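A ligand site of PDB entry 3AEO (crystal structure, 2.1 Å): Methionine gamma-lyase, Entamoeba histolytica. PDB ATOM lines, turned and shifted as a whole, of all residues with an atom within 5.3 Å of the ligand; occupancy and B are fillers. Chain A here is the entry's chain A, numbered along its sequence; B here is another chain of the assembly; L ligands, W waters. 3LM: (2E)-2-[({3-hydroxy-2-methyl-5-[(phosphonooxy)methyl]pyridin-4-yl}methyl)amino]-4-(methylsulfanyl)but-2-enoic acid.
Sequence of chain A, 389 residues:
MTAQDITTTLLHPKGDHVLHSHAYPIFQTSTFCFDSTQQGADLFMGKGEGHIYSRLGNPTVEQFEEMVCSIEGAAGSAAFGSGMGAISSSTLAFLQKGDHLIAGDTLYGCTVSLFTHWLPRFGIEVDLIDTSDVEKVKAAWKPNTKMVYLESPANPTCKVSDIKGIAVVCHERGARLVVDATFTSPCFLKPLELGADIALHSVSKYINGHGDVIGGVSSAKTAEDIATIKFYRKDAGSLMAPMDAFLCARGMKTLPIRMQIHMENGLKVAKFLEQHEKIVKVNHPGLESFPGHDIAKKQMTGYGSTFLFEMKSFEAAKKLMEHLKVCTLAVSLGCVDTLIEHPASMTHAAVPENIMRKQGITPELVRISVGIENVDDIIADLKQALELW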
ATOM      1  N   SER A  82     -30.896 -14.947  13.842  1.00  0.00           N
ATOM      2  CA  SER A  82     -29.794 -15.921  13.746  1.00  0.00           C
ATOM      3  C   SER A  82     -29.757 -16.465  12.315  1.00  0.00           C
ATOM      4  O   SER A  82     -30.749 -16.360  11.611  1.00  0.00           O
ATOM      5  CB  SER A  82     -29.983 -17.073  14.715  1.00  0.00           C
ATOM      6  OG  SER A  82     -31.199 -17.745  14.483  1.00  0.00           O
ATOM      7  N   GLY A  83     -28.626 -17.044  11.910  1.00  0.00           N
ATOM      8  CA  GLY A  83     -28.541 -17.809  10.673  1.00  0.00           C
ATOM      9  C   GLY A  83     -29.683 -18.823  10.584  1.00  0.00           C
ATOM     10  O   GLY A  83     -30.307 -18.984   9.529  1.00  0.00           O
ATOM     11  N   MET A  84     -29.945 -19.536  11.683  1.00  0.00           N
ATOM     12  CA  MET A  84     -30.990 -20.542  11.662  1.00  0.00           C
ATOM     13  C   MET A  84     -32.368 -19.909  11.399  1.00  0.00           C
ATOM     14  O   MET A  84     -33.200 -20.546  10.744  1.00  0.00           O
ATOM     15  CB  MET A  84     -31.003 -21.401  12.958  1.00  0.00           C
ATOM     16  CG  MET A  84     -29.804 -22.378  13.133  1.00  0.00           C
ATOM     17  SD  MET A  84     -29.329 -23.306  11.634  1.00  0.00           S
ATOM     18  CE  MET A  84     -30.857 -24.187  11.297  1.00  0.00           C
ATOM     19  N   GLY A  85     -32.625 -18.695  11.909  1.00  0.00           N
ATOM     20  CA  GLY A  85     -33.853 -17.977  11.581  1.00  0.00           C
ATOM     21  C   GLY A  85     -33.917 -17.704  10.061  1.00  0.00           C
ATOM     22  O   GLY A  85     -34.971 -17.820   9.467  1.00  0.00           O
ATOM     23  N   ILE A  87     -32.438 -19.468   7.673  1.00  0.00           N
ATOM     24  CA  ILE A  87     -32.614 -20.772   7.011  1.00  0.00           C
ATOM     25  C   ILE A  87     -34.044 -21.319   7.142  1.00  0.00           C
ATOM     26  O   ILE A  87     -34.619 -21.736   6.144  1.00  0.00           O
ATOM     27  CB  ILE A  87     -31.619 -21.813   7.540  1.00  0.00           C
ATOM     28  CG1 ILE A  87     -30.190 -21.429   7.152  1.00  0.00           C
ATOM     29  CG2 ILE A  87     -31.955 -23.239   7.013  1.00  0.00           C
ATOM     30  CD1 ILE A  87     -29.125 -22.193   8.015  1.00  0.00           C
ATOM     31  N   TYR A 108     -24.045 -27.713   7.910  1.00  0.00           N
ATOM     32  CA  TYR A 108     -24.032 -27.287   9.298  1.00  0.00           C
ATOM     33  C   TYR A 108     -24.974 -28.168  10.167  1.00  0.00           C
ATOM     34  O   TYR A 108     -26.089 -28.519   9.759  1.00  0.00           O
ATOM     35  CB  TYR A 108     -24.386 -25.787   9.409  1.00  0.00           C
ATOM     36  CG  TYR A 108     -24.459 -25.374  10.857  1.00  0.00           C
ATOM     37  CD1 TYR A 108     -23.364 -25.552  11.695  1.00  0.00           C
ATOM     38  CD2 TYR A 108     -25.644 -24.872  11.394  1.00  0.00           C
ATOM     39  CE1 TYR A 108     -23.437 -25.210  13.069  1.00  0.00           C
ATOM     40  CE2 TYR A 108     -25.726 -24.513  12.742  1.00  0.00           C
ATOM     41  CZ  TYR A 108     -24.621 -24.679  13.573  1.00  0.00           C
ATOM     42  OH  TYR A 108     -24.709 -24.354  14.908  1.00  0.00           O
ATOM     43  N   THR A 111     -28.637 -27.232  10.785  1.00  0.00           N
ATOM     44  CA  THR A 111     -29.406 -27.339   9.513  1.00  0.00           C
ATOM     45  C   THR A 111     -29.804 -28.807   9.320  1.00  0.00           C
ATOM     46  O   THR A 111     -30.951 -29.123   8.988  1.00  0.00           O
ATOM     47  CB  THR A 111     -28.609 -26.793   8.330  1.00  0.00           C
ATOM     48  OG1 THR A 111     -28.206 -25.450   8.640  1.00  0.00           O
ATOM     49  CG2 THR A 111     -29.460 -26.795   7.040  1.00  0.00           C
ATOM     50  N   GLU A 151     -25.136 -25.756   0.533  1.00  0.00           N
ATOM     51  CA  GLU A 151     -24.122 -25.035   1.299  1.00  0.00           C
ATOM     52  C   GLU A 151     -22.864 -25.397   0.535  1.00  0.00           C
ATOM     53  O   GLU A 151     -22.536 -26.575   0.436  1.00  0.00           O
ATOM     54  CB  GLU A 151     -24.064 -25.673   2.682  1.00  0.00           C
ATOM     55  CG  GLU A 151     -23.731 -24.818   3.780  1.00  0.00           C
ATOM     56  CD  GLU A 151     -23.585 -25.581   5.104  1.00  0.00           C
ATOM     57  OE1 GLU A 151     -22.429 -25.801   5.493  1.00  0.00           O
ATOM     58  OE2 GLU A 151     -24.606 -25.930   5.774  1.00  0.00           O
ATOM     59  N   ASN A 155     -19.951 -26.878   5.467  1.00  0.00           N
ATOM     60  CA  ASN A 155     -19.422 -26.860   6.799  1.00  0.00           C
ATOM     61  C   ASN A 155     -19.520 -28.327   7.304  1.00  0.00           C
ATOM     62  O   ASN A 155     -20.620 -28.889   7.328  1.00  0.00           O
ATOM     63  CB  ASN A 155     -20.277 -25.895   7.613  1.00  0.00           C
ATOM     64  CG  ASN A 155     -19.819 -25.764   9.053  1.00  0.00           C
ATOM     65  OD1 ASN A 155     -18.928 -26.486   9.500  1.00  0.00           O
ATOM     66  ND2 ASN A 155     -20.440 -24.824   9.808  1.00  0.00           N
ATOM     67  N   ASP A 180     -26.796 -21.316   1.071  1.00  0.00           N
ATOM     68  CA  ASP A 180     -26.115 -20.787   2.257  1.00  0.00           C
ATOM     69  C   ASP A 180     -24.668 -20.500   1.920  1.00  0.00           C
ATOM     70  O   ASP A 180     -23.860 -21.421   1.728  1.00  0.00           O
ATOM     71  CB  ASP A 180     -26.193 -21.804   3.386  1.00  0.00           C
ATOM     72  CG  ASP A 180     -25.623 -21.275   4.705  1.00  0.00           C
ATOM     73  OD1 ASP A 180     -24.930 -20.211   4.715  1.00  0.00           O
ATOM     74  OD2 ASP A 180     -25.859 -21.956   5.737  1.00  0.00           O
ATOM     75  N   THR A 182     -22.569 -18.567   3.849  1.00  0.00           N
ATOM     76  CA  THR A 182     -21.890 -18.182   5.105  1.00  0.00           C
ATOM     77  C   THR A 182     -20.362 -18.335   5.052  1.00  0.00           C
ATOM     78  O   THR A 182     -19.652 -17.411   5.469  1.00  0.00           O
ATOM     79  CB  THR A 182     -22.427 -19.056   6.272  1.00  0.00           C
ATOM     80  OG1 THR A 182     -23.820 -18.781   6.468  1.00  0.00           O
ATOM     81  CG2 THR A 182     -21.639 -18.832   7.598  1.00  0.00           C
ATOM     82  N   PHE A 183     -19.864 -19.469   4.528  1.00  0.00           N
ATOM     83  CA  PHE A 183     -18.445 -19.847   4.610  1.00  0.00           C
ATOM     84  C   PHE A 183     -17.543 -19.016   3.710  1.00  0.00           C
ATOM     85  O   PHE A 183     -16.305 -18.976   3.900  1.00  0.00           O
ATOM     86  CB  PHE A 183     -18.270 -21.329   4.269  1.00  0.00           C
ATOM     87  CG  PHE A 183     -17.886 -22.211   5.442  1.00  0.00           C
ATOM     88  CD1 PHE A 183     -18.551 -22.106   6.675  1.00  0.00           C
ATOM     89  CD2 PHE A 183     -16.904 -23.182   5.293  1.00  0.00           C
ATOM     90  CE1 PHE A 183     -18.208 -22.971   7.744  1.00  0.00           C
ATOM     91  CE2 PHE A 183     -16.559 -24.033   6.362  1.00  0.00           C
ATOM     92  CZ  PHE A 183     -17.203 -23.910   7.570  1.00  0.00           C
ATOM     93  N   SER A 202     -25.360 -16.868   7.796  1.00  0.00           N
ATOM     94  CA  SER A 202     -25.236 -16.530   9.171  1.00  0.00           C
ATOM     95  C   SER A 202     -24.352 -15.260   9.221  1.00  0.00           C
ATOM     96  O   SER A 202     -23.119 -15.322   8.993  1.00  0.00           O
ATOM     97  CB  SER A 202     -24.542 -17.650   9.956  1.00  0.00           C
ATOM     98  OG  SER A 202     -24.355 -17.245  11.295  1.00  0.00           O
ATOM     99  N   VAL A 203     -24.969 -14.129   9.581  1.00  0.00           N
ATOM    100  CA  VAL A 203     -24.267 -12.868   9.780  1.00  0.00           C
ATOM    101  C   VAL A 203     -23.324 -12.933  10.960  1.00  0.00           C
ATOM    102  O   VAL A 203     -22.389 -12.129  11.052  1.00  0.00           O
ATOM    103  CB  VAL A 203     -25.332 -11.764   9.918  1.00  0.00           C
ATOM    104  CG1 VAL A 203     -24.744 -10.437  10.217  1.00  0.00           C
ATOM    105  CG2 VAL A 203     -26.075 -11.694   8.551  1.00  0.00           C
ATOM    106  N   SER A 204     -23.548 -13.902  11.844  1.00  0.00           N
ATOM    107  CA  SER A 204     -22.712 -14.140  13.020  1.00  0.00           C
ATOM    108  C   SER A 204     -21.242 -14.414  12.673  1.00  0.00           C
ATOM    109  O   SER A 204     -20.345 -14.307  13.540  1.00  0.00           O
ATOM    110  CB  SER A 204     -23.232 -15.373  13.783  1.00  0.00           C
ATOM    111  OG  SER A 204     -24.665 -15.440  13.760  1.00  0.00           O
ATOM    112  N   LYS A 205     -20.989 -14.795  11.417  1.00  0.00           N
ATOM    113  CA  LYS A 205     -19.624 -15.170  11.039  1.00  0.00           C
ATOM    114  C   LYS A 205     -18.955 -13.941  10.371  1.00  0.00           C
ATOM    115  O   LYS A 205     -18.890 -12.873  11.010  1.00  0.00           O
ATOM    116  CB  LYS A 205     -19.645 -16.423  10.135  1.00  0.00           C
ATOM    117  CG  LYS A 205     -20.555 -17.551  10.609  1.00  0.00           C
ATOM    118  CD  LYS A 205     -20.391 -17.915  12.076  1.00  0.00           C
ATOM    119  CE  LYS A 205     -21.253 -19.122  12.411  1.00  0.00           C
ATOM    120  NZ  LYS A 205     -21.315 -19.260  13.891  1.00  0.00           N
ATOM    121  N   ILE A 214     -25.152 -12.594  17.125  1.00  0.00           N
ATOM    122  CA  ILE A 214     -25.780 -13.697  16.409  1.00  0.00           C
ATOM    123  C   ILE A 214     -26.835 -13.100  15.472  1.00  0.00           C
ATOM    124  O   ILE A 214     -27.681 -12.320  15.926  1.00  0.00           O
ATOM    125  CB  ILE A 214     -26.476 -14.665  17.372  1.00  0.00           C
ATOM    126  CG1 ILE A 214     -25.486 -15.207  18.420  1.00  0.00           C
ATOM    127  CG2 ILE A 214     -27.093 -15.842  16.610  1.00  0.00           C
ATOM    128  CD1 ILE A 214     -24.511 -16.215  17.896  1.00  0.00           C
ATOM    129  N   GLY A 215     -26.825 -13.445  14.177  1.00  0.00           N
ATOM    130  CA  GLY A 215     -27.820 -12.869  13.307  1.00  0.00           C
ATOM    131  C   GLY A 215     -27.836 -13.605  12.004  1.00  0.00           C
ATOM    132  O   GLY A 215     -26.869 -14.347  11.709  1.00  0.00           O
ATOM    133  N   VAL A 331     -16.236 -22.835  19.283  1.00  0.00           N
ATOM    134  CA  VAL A 331     -17.003 -23.022  18.043  1.00  0.00           C
ATOM    135  C   VAL A 331     -17.218 -21.655  17.369  1.00  0.00           C
ATOM    136  O   VAL A 331     -16.757 -20.645  17.889  1.00  0.00           O
ATOM    137  CB  VAL A 331     -18.317 -23.810  18.210  1.00  0.00           C
ATOM    138  CG1 VAL A 331     -18.018 -25.164  18.809  1.00  0.00           C
ATOM    139  CG2 VAL A 331     -19.358 -23.031  19.072  1.00  0.00           C
ATOM    140  N   SER A 332     -17.871 -21.664  16.196  1.00  0.00           N
ATOM    141  CA  SER A 332     -18.051 -20.468  15.345  1.00  0.00           C
ATOM    142  C   SER A 332     -16.857 -20.208  14.437  1.00  0.00           C
ATOM    143  O   SER A 332     -15.871 -20.930  14.461  1.00  0.00           O
ATOM    144  CB  SER A 332     -18.363 -19.210  16.181  1.00  0.00           C
ATOM    145  OG  SER A 332     -18.955 -18.240  15.328  1.00  0.00           O
ATOM    146  N   LEU A 333     -16.946 -19.153  13.620  1.00  0.00           N
ATOM    147  CA  LEU A 333     -15.939 -18.926  12.584  1.00  0.00           C
ATOM    148  C   LEU A 333     -16.123 -17.553  12.040  1.00  0.00           C
ATOM    149  O   LEU A 333     -17.137 -16.895  12.333  1.00  0.00           O
ATOM    150  CB  LEU A 333     -16.086 -19.948  11.434  1.00  0.00           C
ATOM    151  CG  LEU A 333     -17.447 -19.985  10.713  1.00  0.00           C
ATOM    152  CD1 LEU A 333     -17.358 -19.650   9.208  1.00  0.00           C
ATOM    153  CD2 LEU A 333     -18.149 -21.367  10.900  1.00  0.00           C
ATOM    154  N   GLU A 341     -11.592 -25.845  16.378  1.00  0.00           N
ATOM    155  CA  GLU A 341     -12.575 -26.735  17.018  1.00  0.00           C
ATOM    156  C   GLU A 341     -12.468 -28.157  16.439  1.00  0.00           C
ATOM    157  O   GLU A 341     -11.754 -28.398  15.455  1.00  0.00           O
ATOM    158  CB  GLU A 341     -14.024 -26.199  16.889  1.00  0.00           C
ATOM    159  CG  GLU A 341     -14.633 -26.119  15.428  1.00  0.00           C
ATOM    160  CD  GLU A 341     -15.747 -27.173  15.158  1.00  0.00           C
ATOM    161  OE1 GLU A 341     -16.145 -27.385  13.968  1.00  0.00           O
ATOM    162  OE2 GLU A 341     -16.259 -27.774  16.123  1.00  0.00           O
ATOM    163  N   THR A 347     -19.287 -29.041  16.780  1.00  0.00           N
ATOM    164  CA  THR A 347     -20.297 -28.489  15.841  1.00  0.00           C
ATOM    165  C   THR A 347     -21.233 -29.538  15.218  1.00  0.00           C
ATOM    166  O   THR A 347     -22.389 -29.261  14.919  1.00  0.00           O
ATOM    167  CB  THR A 347     -19.663 -27.600  14.713  1.00  0.00           C
ATOM    168  OG1 THR A 347     -18.603 -28.319  14.032  1.00  0.00           O
ATOM    169  CG2 THR A 347     -19.156 -26.275  15.305  1.00  0.00           C
ATOM    170  N   ARG A 367     -11.127 -28.378  12.626  1.00  0.00           N
ATOM    171  CA  ARG A 367     -11.535 -27.272  11.747  1.00  0.00           C
ATOM    172  C   ARG A 367     -10.913 -25.999  12.279  1.00  0.00           C
ATOM    173  O   ARG A 367     -10.981 -25.742  13.474  1.00  0.00           O
ATOM    174  CB  ARG A 367     -13.079 -27.143  11.672  1.00  0.00           C
ATOM    175  CG  ARG A 367     -13.546 -26.158  10.539  1.00  0.00           C
ATOM    176  CD  ARG A 367     -15.015 -25.801  10.656  1.00  0.00           C
ATOM    177  NE  ARG A 367     -15.233 -24.921  11.807  1.00  0.00           N
ATOM    178  CZ  ARG A 367     -16.439 -24.631  12.321  1.00  0.00           C
ATOM    179  NH1 ARG A 367     -17.552 -25.147  11.788  1.00  0.00           N
ATOM    180  NH2 ARG A 367     -16.519 -23.836  13.383  1.00  0.00           N
ATOM    181  N   PHE B  44     -21.368 -30.008  25.050  1.00  0.00           N
ATOM    182  CA  PHE B  44     -22.220 -30.446  23.946  1.00  0.00           C
ATOM    183  C   PHE B  44     -23.090 -31.667  24.305  1.00  0.00           C
ATOM    184  O   PHE B  44     -24.155 -31.845  23.698  1.00  0.00           O
ATOM    185  CB  PHE B  44     -21.390 -30.736  22.686  1.00  0.00           C
ATOM    186  CG  PHE B  44     -21.171 -29.520  21.820  1.00  0.00           C
ATOM    187  CD1 PHE B  44     -19.993 -28.795  21.903  1.00  0.00           C
ATOM    188  CD2 PHE B  44     -22.173 -29.101  20.944  1.00  0.00           C
ATOM    189  CE1 PHE B  44     -19.792 -27.634  21.101  1.00  0.00           C
ATOM    190  CE2 PHE B  44     -21.982 -27.937  20.132  1.00  0.00           C
ATOM    191  CZ  PHE B  44     -20.793 -27.222  20.213  1.00  0.00           C
ATOM    192  N   ILE B  52     -21.509 -22.370  25.450  1.00  0.00           N
ATOM    193  CA  ILE B  52     -20.917 -22.798  24.190  1.00  0.00           C
ATOM    194  C   ILE B  52     -21.041 -21.676  23.165  1.00  0.00           C
ATOM    195  O   ILE B  52     -20.062 -21.311  22.507  1.00  0.00           O
ATOM    196  CB  ILE B  52     -21.625 -24.068  23.641  1.00  0.00           C
ATOM    197  CG1 ILE B  52     -21.465 -25.269  24.617  1.00  0.00           C
ATOM    198  CG2 ILE B  52     -21.107 -24.413  22.202  1.00  0.00           C
ATOM    199  CD1 ILE B  52     -22.516 -26.401  24.398  1.00  0.00           C
ATOM    200  N   TYR B  53     -22.267 -21.163  23.008  1.00  0.00           N
ATOM    201  CA  TYR B  53     -22.605 -20.327  21.850  1.00  0.00           C
ATOM    202  C   TYR B  53     -23.951 -19.695  22.125  1.00  0.00           C
ATOM    203  O   TYR B  53     -24.888 -20.390  22.586  1.00  0.00           O
ATOM    204  CB  TYR B  53     -22.704 -21.220  20.593  1.00  0.00           C
ATOM    205  CG  TYR B  53     -22.931 -20.455  19.287  1.00  0.00           C
ATOM    206  CD1 TYR B  53     -21.888 -19.708  18.678  1.00  0.00           C
ATOM    207  CD2 TYR B  53     -24.150 -20.536  18.619  1.00  0.00           C
ATOM    208  CE1 TYR B  53     -22.086 -19.022  17.446  1.00  0.00           C
ATOM    209  CE2 TYR B  53     -24.358 -19.891  17.370  1.00  0.00           C
ATOM    210  CZ  TYR B  53     -23.321 -19.128  16.809  1.00  0.00           C
ATOM    211  OH  TYR B  53     -23.539 -18.482  15.607  1.00  0.00           O
ATOM    212  N   ARG B  55     -26.681 -18.770  20.680  1.00  0.00           N
ATOM    213  CA  ARG B  55     -27.945 -19.422  20.251  1.00  0.00           C
ATOM    214  C   ARG B  55     -28.350 -20.622  21.168  1.00  0.00           C
ATOM    215  O   ARG B  55     -29.548 -20.871  21.377  1.00  0.00           O
ATOM    216  CB  ARG B  55     -27.903 -19.865  18.777  1.00  0.00           C
ATOM    217  CG  ARG B  55     -29.209 -20.602  18.321  1.00  0.00           C
ATOM    218  CD  ARG B  55     -29.432 -20.549  16.797  1.00  0.00           C
ATOM    219  NE  ARG B  55     -28.188 -20.902  16.117  1.00  0.00           N
ATOM    220  CZ  ARG B  55     -27.627 -22.113  16.047  1.00  0.00           C
ATOM    221  NH1 ARG B  55     -28.225 -23.175  16.595  1.00  0.00           N
ATOM    222  NH2 ARG B  55     -26.464 -22.256  15.417  1.00  0.00           N
ATOM    223  N   LEU B  56     -27.382 -21.362  21.696  1.00  0.00           N
ATOM    224  CA  LEU B  56     -27.694 -22.409  22.694  1.00  0.00           C
ATOM    225  C   LEU B  56     -27.938 -21.816  24.104  1.00  0.00           C
ATOM    226  O   LEU B  56     -28.621 -22.431  24.941  1.00  0.00           O
ATOM    227  CB  LEU B  56     -26.562 -23.464  22.730  1.00  0.00           C
ATOM    228  CG  LEU B  56     -26.084 -24.106  21.424  1.00  0.00           C
ATOM    229  CD1 LEU B  56     -25.076 -25.261  21.642  1.00  0.00           C
ATOM    230  CD2 LEU B  56     -27.243 -24.631  20.629  1.00  0.00           C
HETATM  231  C   3LM L   1     -20.190 -23.384  13.595  1.00  0.00           C
HETATM  232  N   3LM L   1     -21.998 -22.355  12.454  1.00  0.00           N
HETATM  233  O1  3LM L   1     -19.284 -23.212  14.418  1.00  0.00           O
HETATM  234  P   3LM L   1     -26.354 -19.017  13.452  1.00  0.00           P
HETATM  235  N1  3LM L   1     -24.991 -21.829   8.233  1.00  0.00           N
HETATM  236  C2  3LM L   1     -23.716 -22.171   8.349  1.00  0.00           C
HETATM  237  C3  3LM L   1     -23.051 -22.130   9.685  1.00  0.00           C
HETATM  238  O3  3LM L   1     -21.744 -22.486   9.778  1.00  0.00           O
HETATM  239  C4  3LM L   1     -23.848 -21.731  10.857  1.00  0.00           C
HETATM  240  C5  3LM L   1     -25.258 -21.425  10.595  1.00  0.00           C
HETATM  241  C6  3LM L   1     -25.752 -21.493   9.280  1.00  0.00           C
HETATM  242  CA  3LM L   1     -21.456 -22.664  13.676  1.00  0.00           C
HETATM  243  CB  3LM L   1     -22.099 -22.361  14.850  1.00  0.00           C
HETATM  244  SD  3LM L   1     -22.077 -24.363  16.780  1.00  0.00           S
HETATM  245  CE  3LM L   1     -23.230 -24.406  18.107  1.00  0.00           C
HETATM  246  CG  3LM L   1     -21.643 -22.691  16.277  1.00  0.00           C
HETATM  247  C2A 3LM L   1     -22.859 -22.568   7.180  1.00  0.00           C
HETATM  248  C4A 3LM L   1     -23.291 -21.699  12.272  1.00  0.00           C
HETATM  249  C5A 3LM L   1     -26.184 -21.013  11.734  1.00  0.00           C
HETATM  250  OP1 3LM L   1     -27.730 -19.425  13.726  1.00  0.00           O
HETATM  251  OP2 3LM L   1     -25.350 -19.689  14.322  1.00  0.00           O
HETATM  252  OP3 3LM L   1     -26.114 -17.519  13.260  1.00  0.00           O
HETATM  253  OP4 3LM L   1     -25.977 -19.637  12.009  1.00  0.00           O
HETATM  254  O2  3LM L   1     -20.028 -24.161  12.627  1.00  0.00           O
HETATM  255  O   HOH W   1     -20.819 -23.838   4.663  1.00  0.00           O
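Merely in contact with the ligand: Ser 82, Ile 87, Glu 151, Thr 182, Ile 214, Gly 215, Val 331, Leu 333 and Thr 347.
Hydrophobic or aromatic side chains within 4 Å of the ligand: Met 84, Ile 87, Tyr 108, Ile 214, Val 331, Leu 333 and Tyr 53 of chain B.
Within 4 Å of the ligand: Ser 82, Gly 83, Met 84, Ile 87, Tyr 108, Glu 151, Asn 155, Asp 180, Thr 182, Ser 202, Ser 204, Lys 205, Ile 214, Gly 215, Val 331, Ser 332, Leu 333, Thr 347, Arg 367, Tyr 53 of chain B and Arg 55 of chain B.
The nearest printed residue that does not touch the ligand is Leu 56 of chain B (4.1 Å).
N of Ser 332 sits at hydrogen-bond distance from O1 of the ligand (2.7 Å).
The guanidinium group (NE) of Arg 55 of chain B lies within salt-bridge range of an oxygen (OP1) of the ligand.
N of the ligand lies close to NZ of Lys 205 (3.5 Å).
The guanidinium group (NH1) of Arg 367 lies within salt-bridge range of an oxygen (O2) of the ligand (2.8 Å).
OH of Tyr 108 sits close to SD of the ligand (3.2 Å).
An oxygen (OP1) of the ligand lies within hydrogen-bond range of the backbone NH of Met 84 (3.0 Å).
O3 of the ligand lies within hydrogen-bond range of ND2 of Asn 155 (2.7 Å).
The side-chain carboxylate (OD2) of Asp 180 lies within hydrogen-bond range of a nitrogen (N1) of the ligand, 2.6 Å away.
An oxygen (OP2) of the ligand lies within hydrogen-bond range of the side-chain hydroxyl (OH) of Tyr 53 of chain B, 2.5 Å away.
OG of Ser 202 sits at hydrogen-bond distance from OP3 of the ligand (2.7 Å).
OG of Ser 204 sits at hydrogen-bond distance from OP3 of the ligand.
The backbone NH (N) of Gly 83 is in hydrogen-bond range of an oxygen (OP3) of the ligand (2.9 Å).
The backbone NH (N) of Val 203 is in hydrogen-bond range of the backbone carbonyl oxygen (O) of Gly 215 (2.9 Å).
N of Gly 83 is in hydrogen-bond range of O of Gly 215 (3.2 Å).
N of Gly 85 lies within hydrogen-bond range of OG of Ser 82 (3.1 Å).
The backbone NH (N) of Asn 155 lies within hydrogen-bond range of the side-chain carboxylate (OE1) of Glu 151 (2.7 Å).
O of Ser 332 sits at hydrogen-bond distance from NH2 of Arg 367.
The side-chain hydroxyl (OG) of Ser 332 sits at hydrogen-bond distance from the side-chain amino group (NZ) of Lys 205 (2.9 Å).
The side-chain hydroxyl (OH) of Tyr 53 of chain B is in hydrogen-bond range of the side-chain amino group (NZ) of Lys 205, 2.9 Å away.
The guanidinium group of Arg 55 of chain B lies within hydrogen-bond range of the side-chain hydroxyl of Tyr 108 (2.8 Å).
Water W1 bridges OE1 of Glu 151 (2.7 Å) and N of Asn 155 (3.3 Å).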
